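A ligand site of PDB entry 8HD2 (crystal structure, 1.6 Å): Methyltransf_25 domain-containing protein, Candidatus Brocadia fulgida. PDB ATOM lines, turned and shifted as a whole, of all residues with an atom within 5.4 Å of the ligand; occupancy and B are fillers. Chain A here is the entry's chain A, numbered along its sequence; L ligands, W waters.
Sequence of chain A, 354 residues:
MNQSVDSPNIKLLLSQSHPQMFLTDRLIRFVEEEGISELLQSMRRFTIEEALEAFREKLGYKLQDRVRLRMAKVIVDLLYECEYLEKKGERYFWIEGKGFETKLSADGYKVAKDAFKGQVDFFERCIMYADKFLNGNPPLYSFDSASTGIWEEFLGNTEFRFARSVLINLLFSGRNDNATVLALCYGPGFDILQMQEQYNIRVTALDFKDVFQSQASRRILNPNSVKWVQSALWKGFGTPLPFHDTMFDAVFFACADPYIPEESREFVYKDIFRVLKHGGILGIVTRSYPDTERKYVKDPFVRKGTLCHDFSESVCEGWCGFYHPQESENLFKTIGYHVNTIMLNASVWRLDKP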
ATOM      1  N   PHE A 143     -22.907  10.087 -14.834  1.00  0.00           N
ATOM      2  CA  PHE A 143     -22.566   9.548 -13.514  1.00  0.00           C
ATOM      3  C   PHE A 143     -21.479   8.489 -13.697  1.00  0.00           C
ATOM      4  O   PHE A 143     -21.686   7.291 -13.535  1.00  0.00           O
ATOM      5  CB  PHE A 143     -23.801   9.023 -12.805  1.00  0.00           C
ATOM      6  CG  PHE A 143     -24.814  10.088 -12.499  1.00  0.00           C
ATOM      7  CD1 PHE A 143     -24.541  11.067 -11.555  1.00  0.00           C
ATOM      8  CD2 PHE A 143     -26.040  10.114 -13.161  1.00  0.00           C
ATOM      9  CE1 PHE A 143     -25.464  12.078 -11.287  1.00  0.00           C
ATOM     10  CE2 PHE A 143     -26.963  11.125 -12.893  1.00  0.00           C
ATOM     11  CZ  PHE A 143     -26.683  12.097 -11.945  1.00  0.00           C
ATOM     12  N   TRP A 151     -20.476  16.757  -9.859  1.00  0.00           N
ATOM     13  CA  TRP A 151     -21.689  16.498  -9.091  1.00  0.00           C
ATOM     14  C   TRP A 151     -21.531  16.910  -7.638  1.00  0.00           C
ATOM     15  O   TRP A 151     -22.497  17.392  -7.030  1.00  0.00           O
ATOM     16  CB  TRP A 151     -22.059  15.014  -9.206  1.00  0.00           C
ATOM     17  CG  TRP A 151     -22.450  14.655 -10.588  1.00  0.00           C
ATOM     18  CD1 TRP A 151     -21.755  13.876 -11.467  1.00  0.00           C
ATOM     19  CD2 TRP A 151     -23.610  15.112 -11.295  1.00  0.00           C
ATOM     20  NE1 TRP A 151     -22.426  13.799 -12.663  1.00  0.00           N
ATOM     21  CE2 TRP A 151     -23.564  14.553 -12.585  1.00  0.00           C
ATOM     22  CE3 TRP A 151     -24.699  15.915 -10.946  1.00  0.00           C
ATOM     23  CZ2 TRP A 151     -24.551  14.783 -13.543  1.00  0.00           C
ATOM     24  CZ3 TRP A 151     -25.678  16.156 -11.898  1.00  0.00           C
ATOM     25  CH2 TRP A 151     -25.605  15.582 -13.181  1.00  0.00           C
ATOM     26  N   LEU A 155     -24.350  19.357  -6.233  1.00  0.00           N
ATOM     27  CA  LEU A 155     -25.311  18.851  -5.270  1.00  0.00           C
ATOM     28  C   LEU A 155     -25.060  19.361  -3.859  1.00  0.00           C
ATOM     29  O   LEU A 155     -25.911  19.167  -2.989  1.00  0.00           O
ATOM     30  CB  LEU A 155     -25.298  17.323  -5.301  1.00  0.00           C
ATOM     31  CG  LEU A 155     -25.765  16.792  -6.667  1.00  0.00           C
ATOM     32  CD1 LEU A 155     -25.510  15.311  -6.792  1.00  0.00           C
ATOM     33  CD2 LEU A 155     -27.238  17.110  -6.887  1.00  0.00           C
ATOM     34  N   ARG A 164     -33.481  19.083   1.447  1.00  0.00           N
ATOM     35  CA  ARG A 164     -33.210  17.833   2.132  1.00  0.00           C
ATOM     36  C   ARG A 164     -33.507  17.943   3.626  1.00  0.00           C
ATOM     37  O   ARG A 164     -34.102  17.042   4.215  1.00  0.00           O
ATOM     38  CB  ARG A 164     -31.754  17.405   1.920  1.00  0.00           C
ATOM     39  CG  ARG A 164     -31.430  16.910   0.527  1.00  0.00           C
ATOM     40  CD  ARG A 164     -30.127  16.132   0.520  1.00  0.00           C
ATOM     41  NE  ARG A 164     -29.420  16.246  -0.752  1.00  0.00           N
ATOM     42  CZ  ARG A 164     -28.589  17.225  -1.075  1.00  0.00           C
ATOM     43  NH1 ARG A 164     -28.372  18.245  -0.257  1.00  0.00           N
ATOM     44  NH2 ARG A 164     -27.981  17.201  -2.261  1.00  0.00           N
ATOM     45  N   LEU A 184     -31.493   5.888  -1.019  1.00  0.00           N
ATOM     46  CA  LEU A 184     -31.547   5.383  -2.386  1.00  0.00           C
ATOM     47  C   LEU A 184     -30.997   6.426  -3.341  1.00  0.00           C
ATOM     48  O   LEU A 184     -31.404   7.583  -3.312  1.00  0.00           O
ATOM     49  CB  LEU A 184     -32.986   5.042  -2.765  1.00  0.00           C
ATOM     50  CG  LEU A 184     -33.232   4.337  -4.102  1.00  0.00           C
ATOM     51  CD1 LEU A 184     -32.398   3.060  -4.177  1.00  0.00           C
ATOM     52  CD2 LEU A 184     -34.718   4.013  -4.181  1.00  0.00           C
ATOM     53  N   CYS A 185     -30.060   6.003  -4.199  1.00  0.00           N
ATOM     54  CA  CYS A 185     -29.450   6.867  -5.203  1.00  0.00           C
ATOM     55  C   CYS A 185     -28.748   8.046  -4.517  1.00  0.00           C
ATOM     56  O   CYS A 185     -29.064   9.215  -4.757  1.00  0.00           O
ATOM     57  CB  CYS A 185     -30.489   7.345  -6.219  1.00  0.00           C
ATOM     58  SG  CYS A 185     -31.369   5.969  -7.026  1.00  0.00           S
ATOM     59  N   TYR A 186     -27.793   7.705  -3.647  1.00  0.00           N
ATOM     60  CA  TYR A 186     -27.233   8.705  -2.736  1.00  0.00           C
ATOM     61  C   TYR A 186     -26.117   9.540  -3.332  1.00  0.00           C
ATOM     62  O   TYR A 186     -25.781  10.580  -2.764  1.00  0.00           O
ATOM     63  CB  TYR A 186     -26.744   8.027  -1.440  1.00  0.00           C
ATOM     64  CG  TYR A 186     -25.634   6.997  -1.639  1.00  0.00           C
ATOM     65  CD1 TYR A 186     -24.303   7.380  -1.639  1.00  0.00           C
ATOM     66  CD2 TYR A 186     -25.943   5.654  -1.798  1.00  0.00           C
ATOM     67  CE1 TYR A 186     -23.294   6.451  -1.804  1.00  0.00           C
ATOM     68  CE2 TYR A 186     -24.941   4.715  -1.968  1.00  0.00           C
ATOM     69  CZ  TYR A 186     -23.624   5.116  -1.967  1.00  0.00           C
ATOM     70  OH  TYR A 186     -22.621   4.194  -2.135  1.00  0.00           O
ATOM     71  N   GLY A 187     -25.549   9.141  -4.468  1.00  0.00           N
ATOM     72  CA  GLY A 187     -24.559   9.967  -5.129  1.00  0.00           C
ATOM     73  C   GLY A 187     -23.408  10.359  -4.208  1.00  0.00           C
ATOM     74  O   GLY A 187     -22.841   9.504  -3.523  1.00  0.00           O
ATOM     75  N   PRO A 188     -23.069  11.649  -4.169  1.00  0.00           N
ATOM     76  CA  PRO A 188     -21.940  12.098  -3.325  1.00  0.00           C
ATOM     77  C   PRO A 188     -22.183  11.970  -1.814  1.00  0.00           C
ATOM     78  O   PRO A 188     -21.259  12.265  -1.046  1.00  0.00           O
ATOM     79  CB  PRO A 188     -21.769  13.573  -3.710  1.00  0.00           C
ATOM     80  CG  PRO A 188     -22.499  13.736  -4.995  1.00  0.00           C
ATOM     81  CD  PRO A 188     -23.629  12.749  -4.967  1.00  0.00           C
ATOM     82  N   PHE A 190     -24.489  13.671   0.215  1.00  0.00           N
ATOM     83  CA  PHE A 190     -25.043  14.791   0.973  1.00  0.00           C
ATOM     84  C   PHE A 190     -26.319  14.400   1.699  1.00  0.00           C
ATOM     85  O   PHE A 190     -26.587  14.907   2.800  1.00  0.00           O
ATOM     86  CB  PHE A 190     -25.315  15.975   0.038  1.00  0.00           C
ATOM     87  CG  PHE A 190     -24.073  16.604  -0.500  1.00  0.00           C
ATOM     88  CD1 PHE A 190     -23.223  17.328   0.326  1.00  0.00           C
ATOM     89  CD2 PHE A 190     -23.734  16.468  -1.842  1.00  0.00           C
ATOM     90  CE1 PHE A 190     -22.065  17.893  -0.177  1.00  0.00           C
ATOM     91  CE2 PHE A 190     -22.576  17.029  -2.354  1.00  0.00           C
ATOM     92  CZ  PHE A 190     -21.748  17.753  -1.516  1.00  0.00           C
ATOM     93  N   ASP A 191     -27.114  13.494   1.123  1.00  0.00           N
ATOM     94  CA  ASP A 191     -28.340  13.077   1.795  1.00  0.00           C
ATOM     95  C   ASP A 191     -28.029  12.262   3.051  1.00  0.00           C
ATOM     96  O   ASP A 191     -28.596  12.518   4.119  1.00  0.00           O
ATOM     97  CB  ASP A 191     -29.238  12.290   0.832  1.00  0.00           C
ATOM     98  CG  ASP A 191     -28.500  11.235   0.004  1.00  0.00           C
ATOM     99  OD1 ASP A 191     -27.285  10.970   0.204  1.00  0.00           O
ATOM    100  OD2 ASP A 191     -29.159  10.676  -0.890  1.00  0.00           O
ATOM    101  N   ASP A 207     -26.750   2.703  -4.623  1.00  0.00           N
ATOM    102  CA  ASP A 207     -26.766   3.490  -5.851  1.00  0.00           C
ATOM    103  C   ASP A 207     -26.582   2.531  -7.021  1.00  0.00           C
ATOM    104  O   ASP A 207     -26.176   1.381  -6.848  1.00  0.00           O
ATOM    105  CB  ASP A 207     -25.653   4.556  -5.843  1.00  0.00           C
ATOM    106  CG  ASP A 207     -25.991   5.774  -6.683  1.00  0.00           C
ATOM    107  OD1 ASP A 207     -26.784   5.625  -7.634  1.00  0.00           O
ATOM    108  OD2 ASP A 207     -25.456   6.868  -6.396  1.00  0.00           O
ATOM    109  N   PHE A 208     -26.890   2.992  -8.241  1.00  0.00           N
ATOM    110  CA  PHE A 208     -26.734   2.064  -9.360  1.00  0.00           C
ATOM    111  C   PHE A 208     -25.311   2.012  -9.895  1.00  0.00           C
ATOM    112  O   PHE A 208     -25.015   1.134 -10.710  1.00  0.00           O
ATOM    113  CB  PHE A 208     -27.759   2.365 -10.472  1.00  0.00           C
ATOM    114  CG  PHE A 208     -27.355   3.429 -11.485  1.00  0.00           C
ATOM    115  CD1 PHE A 208     -26.906   4.684 -11.082  1.00  0.00           C
ATOM    116  CD2 PHE A 208     -27.506   3.186 -12.838  1.00  0.00           C
ATOM    117  CE1 PHE A 208     -26.576   5.645 -12.016  1.00  0.00           C
ATOM    118  CE2 PHE A 208     -27.168   4.147 -13.783  1.00  0.00           C
ATOM    119  CZ  PHE A 208     -26.699   5.382 -13.369  1.00  0.00           C
ATOM    120  N   LYS A 209     -24.433   2.905  -9.461  1.00  0.00           N
ATOM    121  CA  LYS A 209     -23.009   2.811  -9.721  1.00  0.00           C
ATOM    122  C   LYS A 209     -22.248   3.034  -8.423  1.00  0.00           C
ATOM    123  O   LYS A 209     -22.773   3.638  -7.480  1.00  0.00           O
ATOM    124  CB  LYS A 209     -22.586   3.794 -10.804  1.00  0.00           C
ATOM    125  CG  LYS A 209     -23.299   3.546 -12.123  1.00  0.00           C
ATOM    126  CD  LYS A 209     -23.028   4.630 -13.137  1.00  0.00           C
ATOM    127  CE  LYS A 209     -23.453   4.186 -14.529  1.00  0.00           C
ATOM    128  NZ  LYS A 209     -22.868   2.854 -14.860  1.00  0.00           N
ATOM    129  N   PHE A 212     -19.300   6.954  -6.560  1.00  0.00           N
ATOM    130  CA  PHE A 212     -19.277   7.972  -5.513  1.00  0.00           C
ATOM    131  C   PHE A 212     -18.983   7.412  -4.124  1.00  0.00           C
ATOM    132  O   PHE A 212     -18.899   8.205  -3.180  1.00  0.00           O
ATOM    133  CB  PHE A 212     -20.638   8.681  -5.422  1.00  0.00           C
ATOM    134  CG  PHE A 212     -20.932   9.641  -6.530  1.00  0.00           C
ATOM    135  CD1 PHE A 212     -20.322  10.879  -6.598  1.00  0.00           C
ATOM    136  CD2 PHE A 212     -21.885   9.316  -7.488  1.00  0.00           C
ATOM    137  CE1 PHE A 212     -20.638  11.784  -7.607  1.00  0.00           C
ATOM    138  CE2 PHE A 212     -22.202  10.203  -8.498  1.00  0.00           C
ATOM    139  CZ  PHE A 212     -21.578  11.445  -8.557  1.00  0.00           C
ATOM    140  N   TRP A 234     -27.701  -3.995  -8.065  1.00  0.00           N
ATOM    141  CA  TRP A 234     -28.866  -3.248  -8.544  1.00  0.00           C
ATOM    142  C   TRP A 234     -28.514  -2.511  -9.833  1.00  0.00           C
ATOM    143  O   TRP A 234     -27.762  -1.536  -9.811  1.00  0.00           O
ATOM    144  CB  TRP A 234     -29.349  -2.264  -7.480  1.00  0.00           C
ATOM    145  CG  TRP A 234     -30.684  -1.655  -7.826  1.00  0.00           C
ATOM    146  CD1 TRP A 234     -31.821  -2.332  -8.177  1.00  0.00           C
ATOM    147  CD2 TRP A 234     -31.024  -0.264  -7.847  1.00  0.00           C
ATOM    148  NE1 TRP A 234     -32.836  -1.428  -8.422  1.00  0.00           N
ATOM    149  CE2 TRP A 234     -32.377  -0.157  -8.223  1.00  0.00           C
ATOM    150  CE3 TRP A 234     -30.312   0.907  -7.567  1.00  0.00           C
ATOM    151  CZ2 TRP A 234     -33.028   1.071  -8.337  1.00  0.00           C
ATOM    152  CZ3 TRP A 234     -30.957   2.128  -7.679  1.00  0.00           C
ATOM    153  CH2 TRP A 234     -32.312   2.201  -8.058  1.00  0.00           C
ATOM    154  N   LYS A 235     -29.120  -2.940 -10.936  1.00  0.00           N
ATOM    155  CA  LYS A 235     -28.853  -2.293 -12.211  1.00  0.00           C
ATOM    156  C   LYS A 235     -29.438  -0.882 -12.278  1.00  0.00           C
ATOM    157  O   LYS A 235     -29.003  -0.101 -13.123  1.00  0.00           O
ATOM    158  CB  LYS A 235     -29.399  -3.128 -13.363  1.00  0.00           C
ATOM    159  CG  LYS A 235     -28.470  -4.260 -13.803  1.00  0.00           C
ATOM    160  CD  LYS A 235     -27.293  -3.700 -14.590  1.00  0.00           C
ATOM    161  CE  LYS A 235     -26.397  -4.781 -15.150  1.00  0.00           C
ATOM    162  NZ  LYS A 235     -25.170  -4.223 -15.787  1.00  0.00           N
ATOM    163  N   GLY A 236     -30.404  -0.569 -11.404  1.00  0.00           N
ATOM    164  CA  GLY A 236     -31.004   0.759 -11.403  1.00  0.00           C
ATOM    165  C   GLY A 236     -32.489   0.755 -11.695  1.00  0.00           C
ATOM    166  O   GLY A 236     -33.151  -0.297 -11.605  1.00  0.00           O
ATOM    167  N   PHE A 237     -33.019   1.908 -12.099  1.00  0.00           N
ATOM    168  CA  PHE A 237     -34.457   2.050 -12.266  1.00  0.00           C
ATOM    169  C   PHE A 237     -35.001   1.023 -13.253  1.00  0.00           C
ATOM    170  O   PHE A 237     -34.432   0.797 -14.326  1.00  0.00           O
ATOM    171  CB  PHE A 237     -34.798   3.456 -12.741  1.00  0.00           C
ATOM    172  CG  PHE A 237     -34.398   4.532 -11.793  1.00  0.00           C
ATOM    173  CD1 PHE A 237     -34.607   4.388 -10.421  1.00  0.00           C
ATOM    174  CD2 PHE A 237     -33.784   5.686 -12.260  1.00  0.00           C
ATOM    175  CE1 PHE A 237     -34.237   5.393  -9.547  1.00  0.00           C
ATOM    176  CE2 PHE A 237     -33.412   6.702 -11.393  1.00  0.00           C
ATOM    177  CZ  PHE A 237     -33.637   6.543 -10.024  1.00  0.00           C
ATOM    178  N   ALA A 254     -33.779  11.602  -2.918  1.00  0.00           N
ATOM    179  CA  ALA A 254     -33.608  13.021  -3.214  1.00  0.00           C
ATOM    180  C   ALA A 254     -32.886  13.226  -4.538  1.00  0.00           C
ATOM    181  O   ALA A 254     -31.852  12.615  -4.799  1.00  0.00           O
ATOM    182  CB  ALA A 254     -32.815  13.716  -2.098  1.00  0.00           C
ATOM    183  N   CYS A 255     -33.430  14.130  -5.364  1.00  0.00           N
ATOM    184  CA  CYS A 255     -32.799  14.616  -6.593  1.00  0.00           C
ATOM    185  C   CYS A 255     -32.553  13.514  -7.615  1.00  0.00           C
ATOM    186  O   CYS A 255     -31.683  13.667  -8.485  1.00  0.00           O
ATOM    187  CB  CYS A 255     -31.494  15.345  -6.282  1.00  0.00           C
ATOM    188  SG  CYS A 255     -31.678  16.741  -5.114  1.00  0.00           S
ATOM    189  N   ALA A 256     -33.309  12.419  -7.547  1.00  0.00           N
ATOM    190  CA  ALA A 256     -33.159  11.307  -8.472  1.00  0.00           C
ATOM    191  C   ALA A 256     -34.389  11.045  -9.317  1.00  0.00           C
ATOM    192  O   ALA A 256     -34.256  10.446 -10.402  1.00  0.00           O
ATOM    193  CB  ALA A 256     -32.780  10.029  -7.702  1.00  0.00           C
ATOM    194  N   TYR A 259     -34.327  11.378 -13.130  1.00  0.00           N
ATOM    195  CA  TYR A 259     -33.551  10.405 -13.878  1.00  0.00           C
ATOM    196  C   TYR A 259     -34.317   9.097 -14.093  1.00  0.00           C
ATOM    197  O   TYR A 259     -33.767   8.149 -14.672  1.00  0.00           O
ATOM    198  CB  TYR A 259     -32.208  10.141 -13.174  1.00  0.00           C
ATOM    199  CG  TYR A 259     -31.243  11.283 -13.416  1.00  0.00           C
ATOM    200  CD1 TYR A 259     -30.487  11.353 -14.584  1.00  0.00           C
ATOM    201  CD2 TYR A 259     -31.128  12.321 -12.494  1.00  0.00           C
ATOM    202  CE1 TYR A 259     -29.634  12.403 -14.820  1.00  0.00           C
ATOM    203  CE2 TYR A 259     -30.266  13.394 -12.731  1.00  0.00           C
ATOM    204  CZ  TYR A 259     -29.527  13.413 -13.905  1.00  0.00           C
ATOM    205  OH  TYR A 259     -28.667  14.449 -14.180  1.00  0.00           O
HETATM  206  N1  LIG L   1     -29.563  11.707  -3.640  1.00  0.00           N
HETATM  207  C1  LIG L   1     -28.296  12.420  -3.802  1.00  0.00           C
HETATM  208  C2  LIG L   1     -27.760  12.318  -5.241  1.00  0.00           C
HETATM  209  C3  LIG L   1     -28.702  12.921  -6.337  1.00  0.00           C
HETATM  210  S1  LIG L   1     -27.862  12.767  -7.998  1.00  0.00           S
HETATM  211  C4  LIG L   1     -28.505  13.844  -3.348  1.00  0.00           C
HETATM  212  O1  LIG L   1     -27.649  14.711  -3.620  1.00  0.00           O
HETATM  213  O2  LIG L   1     -29.549  14.139  -2.693  1.00  0.00           O
HETATM  214  C5  LIG L   1     -28.727  11.488  -9.007  1.00  0.00           C
HETATM  215  C6  LIG L   1     -28.651  10.151  -8.377  1.00  0.00           C
HETATM  216  O3  LIG L   1     -29.577   9.265  -9.171  1.00  0.00           O
HETATM  217  C7  LIG L   1     -27.304   9.553  -8.461  1.00  0.00           C
HETATM  218  O4  LIG L   1     -27.043   8.819  -7.215  1.00  0.00           O
HETATM  219  C8  LIG L   1     -27.354   8.615  -9.587  1.00  0.00           C
HETATM  220  O5  LIG L   1     -26.411   7.538  -9.417  1.00  0.00           O
HETATM  221  C9  LIG L   1     -28.764   8.114  -9.579  1.00  0.00           C
HETATM  222  N2  LIG L   1     -29.190   7.611 -10.858  1.00  0.00           N
HETATM  223  C10 LIG L   1     -29.070   8.184 -11.954  1.00  0.00           C
HETATM  224  N3  LIG L   1     -29.511   7.489 -12.852  1.00  0.00           N
HETATM  225  C11 LIG L   1     -30.027   6.221 -12.355  1.00  0.00           C
HETATM  226  C12 LIG L   1     -30.620   5.085 -12.859  1.00  0.00           C
HETATM  227  N4  LIG L   1     -30.872   4.884 -14.282  1.00  0.00           N
HETATM  228  N5  LIG L   1     -30.965   4.050 -11.872  1.00  0.00           N
HETATM  229  C13 LIG L   1     -30.650   4.352 -10.460  1.00  0.00           C
HETATM  230  N6  LIG L   1     -30.064   5.495 -10.120  1.00  0.00           N
HETATM  231  C14 LIG L   1     -29.784   6.326 -10.901  1.00  0.00           C
HETATM  232  O   HOH W   1     -25.532  13.489  -2.425  1.00  0.00           O
HETATM  233  O   HOH W   2     -23.785   6.738  -9.542  1.00  0.00           O
HETATM  234  O   HOH W   3     -29.549   7.245 -15.852  1.00  0.00           O
HETATM  235  O   HOH W   4     -32.187   2.172 -15.286  1.00  0.00           O
HETATM  236  O   HOH W   5     -31.621   9.904  -1.916  1.00  0.00           O
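An oxygen (O5) of the ligand is in hydrogen-bond range of the side-chain carboxylate (OD1) of Asp 207 (2.6 Å).
O of Ala 254 lies within hydrogen-bond range of N1 of the ligand (2.7 Å).
O of Cys 185 is in hydrogen-bond range of N1 of the ligand, at 2.8 Å.
The side-chain sulfur (SG) of Cys 185 sits at hydrogen-bond distance from a nitrogen (N6) of the ligand (3.4 Å).
O1 of the ligand lies within salt-bridge range of NH2 of Arg 164 (2.9 Å).
N1 of the ligand lies within salt-bridge range of OD2 of Asp 191 (3.0 Å).
N5 of the ligand is in hydrogen-bond range of N of Phe 237, 3.0 Å away.
N of Gly 187 sits at hydrogen-bond distance from O4 of the ligand (3.1 Å).
The side-chain carboxylate of Asp 207 lies within hydrogen-bond range of the backbone NH of Gly 187 (3.0 Å).
The backbone carbonyl oxygen (O) of Leu 155 sits at hydrogen-bond distance from the guanidinium group (NH2) of Arg 164 (2.9 Å).
O of Gly 236 lies within hydrogen-bond range of NE1 of Trp 234.
Phe 143 touches the ligand (CZ to C5, 3.6 Å).
Leu 155 touches the ligand (CD1 to S1, 3.7 Å).
Tyr 186 touches the ligand.
Phe 208 touches the ligand (CE1 to O5, 3.2 Å).
Trp 234 touches the ligand.
Gly 236 touches the ligand.
Cys 255 touches the ligand.
CB of Ala 256 touches O3 of the ligand, 3.6 Å away.
CB of Tyr 259 touches N3 of the ligand, at 3.8 Å.
Hydrophobic or aromatic side chains that line the ligand: Phe 143, Leu 155, Phe 208, Trp 234, Phe 237, Ala 254, Ala 256 and Tyr 259.
16 residues have an atom within 4 Å of the ligand: Phe 143, Leu 155, Arg 164, Cys 185, Tyr 186, Gly 187, Asp 191, Asp 207, Phe 208, Trp 234, Gly 236, Phe 237, Ala 254, Cys 255, Ala 256 and Tyr 259.
Water W1 lies within hydrogen-bond range of an oxygen (O1) of the ligand, the backbone NH of Phe 190 and the backbone carbonyl oxygen of Tyr 186.
Water W4 bridges O of Phe 237 (2.8 Å) and N4 of the ligand (3.2 Å).
Water W5 lies within hydrogen-bond range of O of Leu 184 (2.7 Å), OD2 of Asp 191 (2.8 Å), N of Ala 254 (2.9 Å) and N1 of the ligand (3.2 Å).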
